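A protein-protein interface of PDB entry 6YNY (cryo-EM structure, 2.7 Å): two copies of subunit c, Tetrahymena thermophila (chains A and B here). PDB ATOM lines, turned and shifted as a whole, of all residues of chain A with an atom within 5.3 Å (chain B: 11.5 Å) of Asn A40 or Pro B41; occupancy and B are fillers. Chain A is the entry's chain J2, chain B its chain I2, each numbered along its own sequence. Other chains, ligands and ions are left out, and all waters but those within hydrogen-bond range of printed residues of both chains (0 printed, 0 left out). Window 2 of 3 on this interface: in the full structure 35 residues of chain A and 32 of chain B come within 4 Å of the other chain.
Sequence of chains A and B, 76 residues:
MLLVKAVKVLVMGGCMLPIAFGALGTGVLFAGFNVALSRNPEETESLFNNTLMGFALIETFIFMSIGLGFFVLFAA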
ATOM      1  N   ALA A  36     -34.586  24.420  24.475  1.00  0.00           N
ATOM      2  CA  ALA A  36     -33.134  24.537  24.428  1.00  0.00           C
ATOM      3  C   ALA A  36     -32.685  25.929  24.854  1.00  0.00           C
ATOM      4  O   ALA A  36     -31.709  26.074  25.600  1.00  0.00           O
ATOM      5  CB  ALA A  36     -32.631  24.216  23.023  1.00  0.00           C
ATOM      6  N   LEU A  37     -33.387  26.965  24.392  1.00  0.00           N
ATOM      7  CA  LEU A  37     -33.034  28.326  24.782  1.00  0.00           C
ATOM      8  C   LEU A  37     -33.173  28.515  26.287  1.00  0.00           C
ATOM      9  O   LEU A  37     -32.311  29.130  26.925  1.00  0.00           O
ATOM     10  CB  LEU A  37     -33.914  29.327  24.032  1.00  0.00           C
ATOM     11  CG  LEU A  37     -33.696  30.809  24.347  1.00  0.00           C
ATOM     12  CD1 LEU A  37     -32.296  31.253  23.975  1.00  0.00           C
ATOM     13  CD2 LEU A  37     -34.728  31.668  23.632  1.00  0.00           C
ATOM     14  N   SER A  38     -34.250  27.987  26.872  1.00  0.00           N
ATOM     15  CA  SER A  38     -34.454  28.132  28.309  1.00  0.00           C
ATOM     16  C   SER A  38     -33.349  27.450  29.102  1.00  0.00           C
ATOM     17  O   SER A  38     -33.019  27.888  30.210  1.00  0.00           O
ATOM     18  CB  SER A  38     -35.816  27.558  28.699  1.00  0.00           C
ATOM     19  OG  SER A  38     -36.860  28.221  28.011  1.00  0.00           O
ATOM     20  N   ARG A  39     -32.766  26.382  28.555  1.00  0.00           N
ATOM     21  CA  ARG A  39     -31.709  25.673  29.267  1.00  0.00           C
ATOM     22  C   ARG A  39     -30.435  26.503  29.329  1.00  0.00           C
ATOM     23  O   ARG A  39     -29.792  26.587  30.382  1.00  0.00           O
ATOM     24  CB  ARG A  39     -31.441  24.330  28.589  1.00  0.00           C
ATOM     25  CG  ARG A  39     -30.335  23.503  29.227  1.00  0.00           C
ATOM     26  CD  ARG A  39     -30.642  23.184  30.679  1.00  0.00           C
ATOM     27  NE  ARG A  39     -29.674  22.251  31.250  1.00  0.00           N
ATOM     28  CZ  ARG A  39     -28.487  22.597  31.737  1.00  0.00           C
ATOM     29  NH1 ARG A  39     -28.099  23.866  31.726  1.00  0.00           N
ATOM     30  NH2 ARG A  39     -27.684  21.669  32.234  1.00  0.00           N
ATOM     31  N   ASN A  40     -30.054  27.122  28.215  1.00  0.00           N
ATOM     32  CA  ASN A  40     -28.823  27.908  28.126  1.00  0.00           C
ATOM     33  C   ASN A  40     -29.092  29.145  27.285  1.00  0.00           C
ATOM     34  O   ASN A  40     -28.727  29.210  26.105  1.00  0.00           O
ATOM     35  CB  ASN A  40     -27.684  27.076  27.535  1.00  0.00           C
ATOM     36  CG  ASN A  40     -26.385  27.846  27.450  1.00  0.00           C
ATOM     37  OD1 ASN A  40     -26.234  28.903  28.062  1.00  0.00           O
ATOM     38  ND2 ASN A  40     -25.435  27.315  26.692  1.00  0.00           N
ATOM     39  N   PRO A  41     -29.731  30.165  27.867  1.00  0.00           N
ATOM     40  CA  PRO A  41     -30.033  31.379  27.095  1.00  0.00           C
ATOM     41  C   PRO A  41     -28.803  32.184  26.716  1.00  0.00           C
ATOM     42  O   PRO A  41     -28.918  33.098  25.888  1.00  0.00           O
ATOM     43  CB  PRO A  41     -30.944  32.174  28.037  1.00  0.00           C
ATOM     44  CG  PRO A  41     -30.573  31.704  29.398  1.00  0.00           C
ATOM     45  CD  PRO A  41     -30.236  30.251  29.248  1.00  0.00           C
ATOM     46  N   GLU A  42     -27.640  31.882  27.293  1.00  0.00           N
ATOM     47  CA  GLU A  42     -26.440  32.654  27.000  1.00  0.00           C
ATOM     48  C   GLU A  42     -26.046  32.566  25.532  1.00  0.00           C
ATOM     49  O   GLU A  42     -25.364  33.467  25.029  1.00  0.00           O
ATOM     50  CB  GLU A  42     -25.286  32.172  27.881  1.00  0.00           C
ATOM     51  CG  GLU A  42     -24.041  33.040  27.807  1.00  0.00           C
ATOM     52  CD  GLU A  42     -22.951  32.578  28.754  1.00  0.00           C
ATOM     53  OE1 GLU A  42     -23.136  31.530  29.408  1.00  0.00           O
ATOM     54  OE2 GLU A  42     -21.911  33.263  28.846  1.00  0.00           O
ATOM     55  N   GLU A  43     -26.455  31.508  24.838  1.00  0.00           N
ATOM     56  CA  GLU A  43     -26.120  31.286  23.437  1.00  0.00           C
ATOM     57  C   GLU A  43     -27.373  31.268  22.568  1.00  0.00           C
ATOM     58  O   GLU A  43     -27.532  30.416  21.692  1.00  0.00           O
ATOM     59  CB  GLU A  43     -25.329  29.991  23.274  1.00  0.00           C
ATOM     60  CG  GLU A  43     -26.053  28.757  23.773  1.00  0.00           C
ATOM     61  CD  GLU A  43     -25.238  27.496  23.586  1.00  0.00           C
ATOM     62  OE1 GLU A  43     -24.096  27.592  23.089  1.00  0.00           O
ATOM     63  OE2 GLU A  43     -25.738  26.406  23.936  1.00  0.00           O
ATOM     64  N   THR A  44     -28.282  32.215  22.809  1.00  0.00           N
ATOM     65  CA  THR A  44     -29.507  32.284  22.016  1.00  0.00           C
ATOM     66  C   THR A  44     -29.198  32.423  20.531  1.00  0.00           C
ATOM     67  O   THR A  44     -29.883  31.829  19.689  1.00  0.00           O
ATOM     68  CB  THR A  44     -30.379  33.447  22.490  1.00  0.00           C
ATOM     69  OG1 THR A  44     -31.632  33.424  21.794  1.00  0.00           O
ATOM     70  CG2 THR A  44     -29.694  34.779  22.230  1.00  0.00           C
ATOM     71  N   LEU A  47     -28.097  28.916  18.952  1.00  0.00           N
ATOM     72  CA  LEU A  47     -29.264  28.055  18.798  1.00  0.00           C
ATOM     73  C   LEU A  47     -30.162  28.547  17.670  1.00  0.00           C
ATOM     74  O   LEU A  47     -30.648  27.752  16.857  1.00  0.00           O
ATOM     75  CB  LEU A  47     -30.049  28.000  20.109  1.00  0.00           C
ATOM     76  CG  LEU A  47     -29.318  27.506  21.357  1.00  0.00           C
ATOM     77  CD1 LEU A  47     -30.169  27.787  22.582  1.00  0.00           C
ATOM     78  CD2 LEU A  47     -28.986  26.026  21.266  1.00  0.00           C
ATOM     79  N   GLY B  32     -32.810  17.721  18.655  1.00  0.00           N
ATOM     80  CA  GLY B  32     -31.885  17.128  19.605  1.00  0.00           C
ATOM     81  C   GLY B  32     -30.548  17.840  19.630  1.00  0.00           C
ATOM     82  O   GLY B  32     -29.929  17.986  20.687  1.00  0.00           O
ATOM     83  N   PHE B  33     -30.081  18.291  18.465  1.00  0.00           N
ATOM     84  CA  PHE B  33     -28.825  19.030  18.411  1.00  0.00           C
ATOM     85  C   PHE B  33     -28.927  20.339  19.179  1.00  0.00           C
ATOM     86  O   PHE B  33     -27.989  20.730  19.883  1.00  0.00           O
ATOM     87  CB  PHE B  33     -28.442  19.288  16.956  1.00  0.00           C
ATOM     88  CG  PHE B  33     -27.361  20.314  16.780  1.00  0.00           C
ATOM     89  CD1 PHE B  33     -27.642  21.533  16.192  1.00  0.00           C
ATOM     90  CD2 PHE B  33     -26.067  20.062  17.199  1.00  0.00           C
ATOM     91  CE1 PHE B  33     -26.655  22.479  16.023  1.00  0.00           C
ATOM     92  CE2 PHE B  33     -25.076  21.007  17.032  1.00  0.00           C
ATOM     93  CZ  PHE B  33     -25.370  22.216  16.443  1.00  0.00           C
ATOM     94  N   ASN B  34     -30.060  21.031  19.059  1.00  0.00           N
ATOM     95  CA  ASN B  34     -30.226  22.295  19.765  1.00  0.00           C
ATOM     96  C   ASN B  34     -30.297  22.077  21.271  1.00  0.00           C
ATOM     97  O   ASN B  34     -29.533  22.681  22.033  1.00  0.00           O
ATOM     98  CB  ASN B  34     -31.478  23.014  19.266  1.00  0.00           C
ATOM     99  CG  ASN B  34     -31.319  23.540  17.856  1.00  0.00           C
ATOM    100  OD1 ASN B  34     -30.209  23.617  17.332  1.00  0.00           O
ATOM    101  ND2 ASN B  34     -32.431  23.919  17.240  1.00  0.00           N
ATOM    102  N   VAL B  35     -31.212  21.216  21.721  1.00  0.00           N
ATOM    103  CA  VAL B  35     -31.349  20.976  23.154  1.00  0.00           C
ATOM    104  C   VAL B  35     -30.055  20.408  23.721  1.00  0.00           C
ATOM    105  O   VAL B  35     -29.627  20.778  24.820  1.00  0.00           O
ATOM    106  CB  VAL B  35     -32.548  20.049  23.426  1.00  0.00           C
ATOM    107  CG1 VAL B  35     -32.248  18.642  22.957  1.00  0.00           C
ATOM    108  CG2 VAL B  35     -32.905  20.058  24.896  1.00  0.00           C
ATOM    109  N   ALA B  36     -29.407  19.507  22.980  1.00  0.00           N
ATOM    110  CA  ALA B  36     -28.144  18.950  23.447  1.00  0.00           C
ATOM    111  C   ALA B  36     -27.053  20.008  23.472  1.00  0.00           C
ATOM    112  O   ALA B  36     -26.180  19.981  24.347  1.00  0.00           O
ATOM    113  CB  ALA B  36     -27.727  17.775  22.564  1.00  0.00           C
ATOM    114  N   LEU B  37     -27.084  20.941  22.519  1.00  0.00           N
ATOM    115  CA  LEU B  37     -26.108  22.023  22.508  1.00  0.00           C
ATOM    116  C   LEU B  37     -26.223  22.874  23.766  1.00  0.00           C
ATOM    117  O   LEU B  37     -25.209  23.264  24.357  1.00  0.00           O
ATOM    118  CB  LEU B  37     -26.300  22.882  21.258  1.00  0.00           C
ATOM    119  CG  LEU B  37     -25.358  24.075  21.093  1.00  0.00           C
ATOM    120  CD1 LEU B  37     -23.918  23.610  20.970  1.00  0.00           C
ATOM    121  CD2 LEU B  37     -25.756  24.903  19.883  1.00  0.00           C
ATOM    122  N   SER B  38     -27.453  23.165  24.193  1.00  0.00           N
ATOM    123  CA  SER B  38     -27.648  23.996  25.375  1.00  0.00           C
ATOM    124  C   SER B  38     -27.065  23.333  26.614  1.00  0.00           C
ATOM    125  O   SER B  38     -26.454  24.002  27.458  1.00  0.00           O
ATOM    126  CB  SER B  38     -29.136  24.277  25.571  1.00  0.00           C
ATOM    127  OG  SER B  38     -29.700  24.843  24.402  1.00  0.00           O
ATOM    128  N   ARG B  39     -27.236  22.017  26.742  1.00  0.00           N
ATOM    129  CA  ARG B  39     -26.773  21.334  27.942  1.00  0.00           C
ATOM    130  C   ARG B  39     -25.252  21.317  28.023  1.00  0.00           C
ATOM    131  O   ARG B  39     -24.692  21.364  29.124  1.00  0.00           O
ATOM    132  CB  ARG B  39     -27.315  19.905  27.968  1.00  0.00           C
ATOM    133  CG  ARG B  39     -28.818  19.809  27.764  1.00  0.00           C
ATOM    134  CD  ARG B  39     -29.426  18.685  28.584  1.00  0.00           C
ATOM    135  NE  ARG B  39     -30.824  18.447  28.235  1.00  0.00           N
ATOM    136  CZ  ARG B  39     -31.633  17.624  28.896  1.00  0.00           C
ATOM    137  NH1 ARG B  39     -31.191  16.956  29.953  1.00  0.00           N
ATOM    138  NH2 ARG B  39     -32.890  17.472  28.502  1.00  0.00           N
ATOM    139  N   ASN B  40     -24.571  21.248  26.882  1.00  0.00           N
ATOM    140  CA  ASN B  40     -23.109  21.225  26.843  1.00  0.00           C
ATOM    141  C   ASN B  40     -22.634  21.961  25.600  1.00  0.00           C
ATOM    142  O   ASN B  40     -22.293  21.348  24.582  1.00  0.00           O
ATOM    143  CB  ASN B  40     -22.574  19.794  26.862  1.00  0.00           C
ATOM    144  CG  ASN B  40     -21.065  19.740  26.929  1.00  0.00           C
ATOM    145  OD1 ASN B  40     -20.414  20.720  27.288  1.00  0.00           O
ATOM    146  ND2 ASN B  40     -20.499  18.591  26.583  1.00  0.00           N
ATOM    147  N   PRO B  41     -22.591  23.296  25.649  1.00  0.00           N
ATOM    148  CA  PRO B  41     -22.121  24.058  24.483  1.00  0.00           C
ATOM    149  C   PRO B  41     -20.621  23.980  24.265  1.00  0.00           C
ATOM    150  O   PRO B  41     -20.142  24.456  23.228  1.00  0.00           O
ATOM    151  CB  PRO B  41     -22.557  25.489  24.808  1.00  0.00           C
ATOM    152  CG  PRO B  41     -22.553  25.539  26.287  1.00  0.00           C
ATOM    153  CD  PRO B  41     -23.016  24.183  26.744  1.00  0.00           C
ATOM    154  N   GLU B  42     -19.870  23.400  25.202  1.00  0.00           N
ATOM    155  CA  GLU B  42     -18.416  23.398  25.093  1.00  0.00           C
ATOM    156  C   GLU B  42     -17.944  22.661  23.845  1.00  0.00           C
ATOM    157  O   GLU B  42     -16.862  22.955  23.324  1.00  0.00           O
ATOM    158  CB  GLU B  42     -17.802  22.770  26.345  1.00  0.00           C
ATOM    159  CG  GLU B  42     -16.294  22.934  26.449  1.00  0.00           C
ATOM    160  CD  GLU B  42     -15.727  22.303  27.706  1.00  0.00           C
ATOM    161  OE1 GLU B  42     -16.506  21.702  28.474  1.00  0.00           O
ATOM    162  OE2 GLU B  42     -14.502  22.408  27.924  1.00  0.00           O
ATOM    163  N   GLU B  43     -18.733  21.707  23.354  1.00  0.00           N
ATOM    164  CA  GLU B  43     -18.388  20.906  22.183  1.00  0.00           C
ATOM    165  C   GLU B  43     -19.303  21.223  21.003  1.00  0.00           C
ATOM    166  O   GLU B  43     -19.712  20.332  20.256  1.00  0.00           O
ATOM    167  CB  GLU B  43     -18.446  19.420  22.517  1.00  0.00           C
ATOM    168  CG  GLU B  43     -19.793  18.954  23.035  1.00  0.00           C
ATOM    169  CD  GLU B  43     -19.875  17.447  23.161  1.00  0.00           C
ATOM    170  OE1 GLU B  43     -18.919  16.761  22.741  1.00  0.00           O
ATOM    171  OE2 GLU B  43     -20.895  16.948  23.680  1.00  0.00           O
ATOM    172  N   THR B  44     -19.632  22.504  20.830  1.00  0.00           N
ATOM    173  CA  THR B  44     -20.544  22.923  19.770  1.00  0.00           C
ATOM    174  C   THR B  44     -20.142  22.346  18.416  1.00  0.00           C
ATOM    175  O   THR B  44     -20.929  21.653  17.762  1.00  0.00           O
ATOM    176  CB  THR B  44     -20.592  24.450  19.704  1.00  0.00           C
ATOM    177  OG1 THR B  44     -20.967  24.974  20.984  1.00  0.00           O
ATOM    178  CG2 THR B  44     -21.589  24.910  18.650  1.00  0.00           C
ATOM    179  N   GLU B  45     -18.913  22.630  17.976  1.00  0.00           N
ATOM    180  CA  GLU B  45     -18.478  22.174  16.659  1.00  0.00           C
ATOM    181  C   GLU B  45     -18.652  20.668  16.503  1.00  0.00           C
ATOM    182  O   GLU B  45     -19.063  20.191  15.438  1.00  0.00           O
ATOM    183  CB  GLU B  45     -17.018  22.575  16.414  1.00  0.00           C
ATOM    184  CG  GLU B  45     -15.971  21.767  17.185  1.00  0.00           C
ATOM    185  CD  GLU B  45     -16.035  21.988  18.685  1.00  0.00           C
ATOM    186  OE1 GLU B  45     -16.941  22.713  19.147  1.00  0.00           O
ATOM    187  OE2 GLU B  45     -15.174  21.438  19.403  1.00  0.00           O
ATOM    188  N   SER B  46     -18.342  19.901  17.550  1.00  0.00           N
ATOM    189  CA  SER B  46     -18.511  18.455  17.478  1.00  0.00           C
ATOM    190  C   SER B  46     -19.958  18.100  17.160  1.00  0.00           C
ATOM    191  O   SER B  46     -20.243  17.394  16.186  1.00  0.00           O
ATOM    192  CB  SER B  46     -18.065  17.809  18.791  1.00  0.00           C
ATOM    193  OG  SER B  46     -18.161  16.397  18.720  1.00  0.00           O
ATOM    194  N   LEU B  47     -20.890  18.590  17.979  1.00  0.00           N
ATOM    195  CA  LEU B  47     -22.305  18.334  17.736  1.00  0.00           C
ATOM    196  C   LEU B  47     -22.711  18.797  16.343  1.00  0.00           C
ATOM    197  O   LEU B  47     -23.404  18.081  15.612  1.00  0.00           O
ATOM    198  CB  LEU B  47     -23.150  19.036  18.798  1.00  0.00           C
ATOM    199  CG  LEU B  47     -22.907  18.668  20.262  1.00  0.00           C
ATOM    200  CD1 LEU B  47     -23.610  19.670  21.158  1.00  0.00           C
ATOM    201  CD2 LEU B  47     -23.385  17.261  20.566  1.00  0.00           C
ATOM    202  N   PHE B  48     -22.281  20.001  15.959  1.00  0.00           N
ATOM    203  CA  PHE B  48     -22.687  20.569  14.677  1.00  0.00           C
ATOM    204  C   PHE B  48     -22.302  19.651  13.526  1.00  0.00           C
ATOM    205  O   PHE B  48     -23.116  19.376  12.636  1.00  0.00           O
ATOM    206  CB  PHE B  48     -22.062  21.951  14.498  1.00  0.00           C
ATOM    207  CG  PHE B  48     -22.617  22.719  13.337  1.00  0.00           C
ATOM    208  CD1 PHE B  48     -23.759  23.486  13.478  1.00  0.00           C
ATOM    209  CD2 PHE B  48     -21.991  22.679  12.105  1.00  0.00           C
ATOM    210  CE1 PHE B  48     -24.271  24.194  12.411  1.00  0.00           C
ATOM    211  CE2 PHE B  48     -22.497  23.386  11.032  1.00  0.00           C
ATOM    212  CZ  PHE B  48     -23.639  24.146  11.187  1.00  0.00           C
ATOM    213  N   ASN B  49     -21.059  19.170  13.521  1.00  0.00           N
ATOM    214  CA  ASN B  49     -20.614  18.297  12.440  1.00  0.00           C
ATOM    215  C   ASN B  49     -21.438  17.016  12.411  1.00  0.00           C
ATOM    216  O   ASN B  49     -21.896  16.583  11.348  1.00  0.00           O
ATOM    217  CB  ASN B  49     -19.125  17.985  12.590  1.00  0.00           C
ATOM    218  CG  ASN B  49     -18.250  19.200  12.358  1.00  0.00           C
ATOM    219  OD1 ASN B  49     -18.712  20.225  11.853  1.00  0.00           O
ATOM    220  ND2 ASN B  49     -16.977  19.091  12.715  1.00  0.00           N
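O of Leu B37 lies close to OE2 of Glu A43, 3.2 Å away.
OG of Ser B38 lies within hydrogen-bond range of O of Ala A36, 2.6 Å away.
Hydrophobic or aromatic side chains of chain B within 4 Å of the printed part of chain A: Leu B37 and Pro B41.
Printed residues of chain A that touch a printed residue of chain B: Ala A36, Arg A39, Asn A40, Glu A43 and Leu A47.
Hydrophobic or aromatic side chains of chain A that line the printed part of chain B: Ala A36 and Leu A47.
Among the printed residues, 12 pairs touch across the chains.
Among the printed residues, no Asp or Glu carboxylate lies within 4 Å of a Lys or Arg side-chain nitrogen of the other chain.
Ala A36 touches Ser B38, but with the chains exchanged Ser A38 does not touch Ala B36 (10.5 Å).
Arg A39 touches Ser B38, but with the chains exchanged Ser A38 does not touch Arg B39 (8.5 Å).
Asn A40 touches Ser B38, but with the chains exchanged Ser A38 does not touch Asn B40 (11.0 Å).
Asn A40 touches Pro B41, but with the chains exchanged Pro A41 does not touch Asn B40 (10.3 Å).
10 positions are printed for both chains.
Among the printed residues, merely in contact across the chains: Ala A36 with Asn B34 (3.6 Å), Ala A36 with Val B35 (3.5 Å), Arg A39 with Ser B38 (3.8 Å), Asn A40 with Ser B38 (3.3 Å), Asn A40 with Pro B41 (3.4 Å), Glu A43 with Ser B38 (3.4 Å), Glu A43 with Pro B41 (3.1 Å), Leu A47 with Asn B34 (3.5 Å), Leu A47 with Leu B37 (3.7 Å) and Leu A47 with Ser B38 (3.4 Å).
Of chain B, only Ser B38 (3.3 Å) and Pro B41 (3.4 Å) come within 4 Å of Asn A40.
Pro B41 touches two residues of chain A.
Of chain B, only Asn B34 (3.6 Å), Val B35 (3.5 Å) and Ser B38 (2.6 Å) come within 4 Å of Ala A36.
No residue of chain B comes within 4 Å of Leu A37.
No residue of chain B comes within 4 Å of Ser A38.
Arg A39 touches just one residue of chain B: Ser B38 (3.8 Å).
No residue of chain B comes within 4 Å of Pro A41.
No residue of chain B comes within 4 Å of Glu A42.
No residue of chain B comes within 4 Å of Thr A44.
Printed residues of chain A within 4 Å of Asn B34: Ala A36 and Leu A47.
Printed residues of chain A within 4 Å of Ser B38: Ala A36 (2.6 Å), Arg A39 (3.8 Å), Asn A40 (3.3 Å), Glu A43 (3.4 Å) and Leu A47 (3.4 Å).
Of the printed residues of chain A, Val B35 touches Ala A36.
Printed residues of chain A within 4 Å of Leu B37: Glu A43 and Leu A47.
Of the printed residues of chain B, Leu A47 touches Asn B34, Leu B37 and Ser B38.
Ala B36 touches none of the printed residues of chain A.
Arg B39 touches none of the printed residues of chain A.
The nearest residue of chain B that does not touch Asn A40 is Leu B37 (4.7 Å).
The nearest printed residue of chain A that does not touch Pro B41 is Glu A42 (6.8 Å).
The nearest printed residue of chain A that does not touch Ser B38 is Leu A37 (4.3 Å).
The backbone carbonyl oxygen of Pro B41 lies within hydrogen-bond range of the side-chain hydroxyl of Thr B44, at 2.4 Å.
OE2 of Glu A43 is in hydrogen-bond range of ND2 of Asn A40 (2.9 Å).
OD1 of Asn A40 sits close to N of Glu A42 (3.4 Å).
The backbone carbonyl oxygen (O) of Asn B34 is in hydrogen-bond range of the side-chain hydroxyl (OG) of Ser B38, 3.2 Å away.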
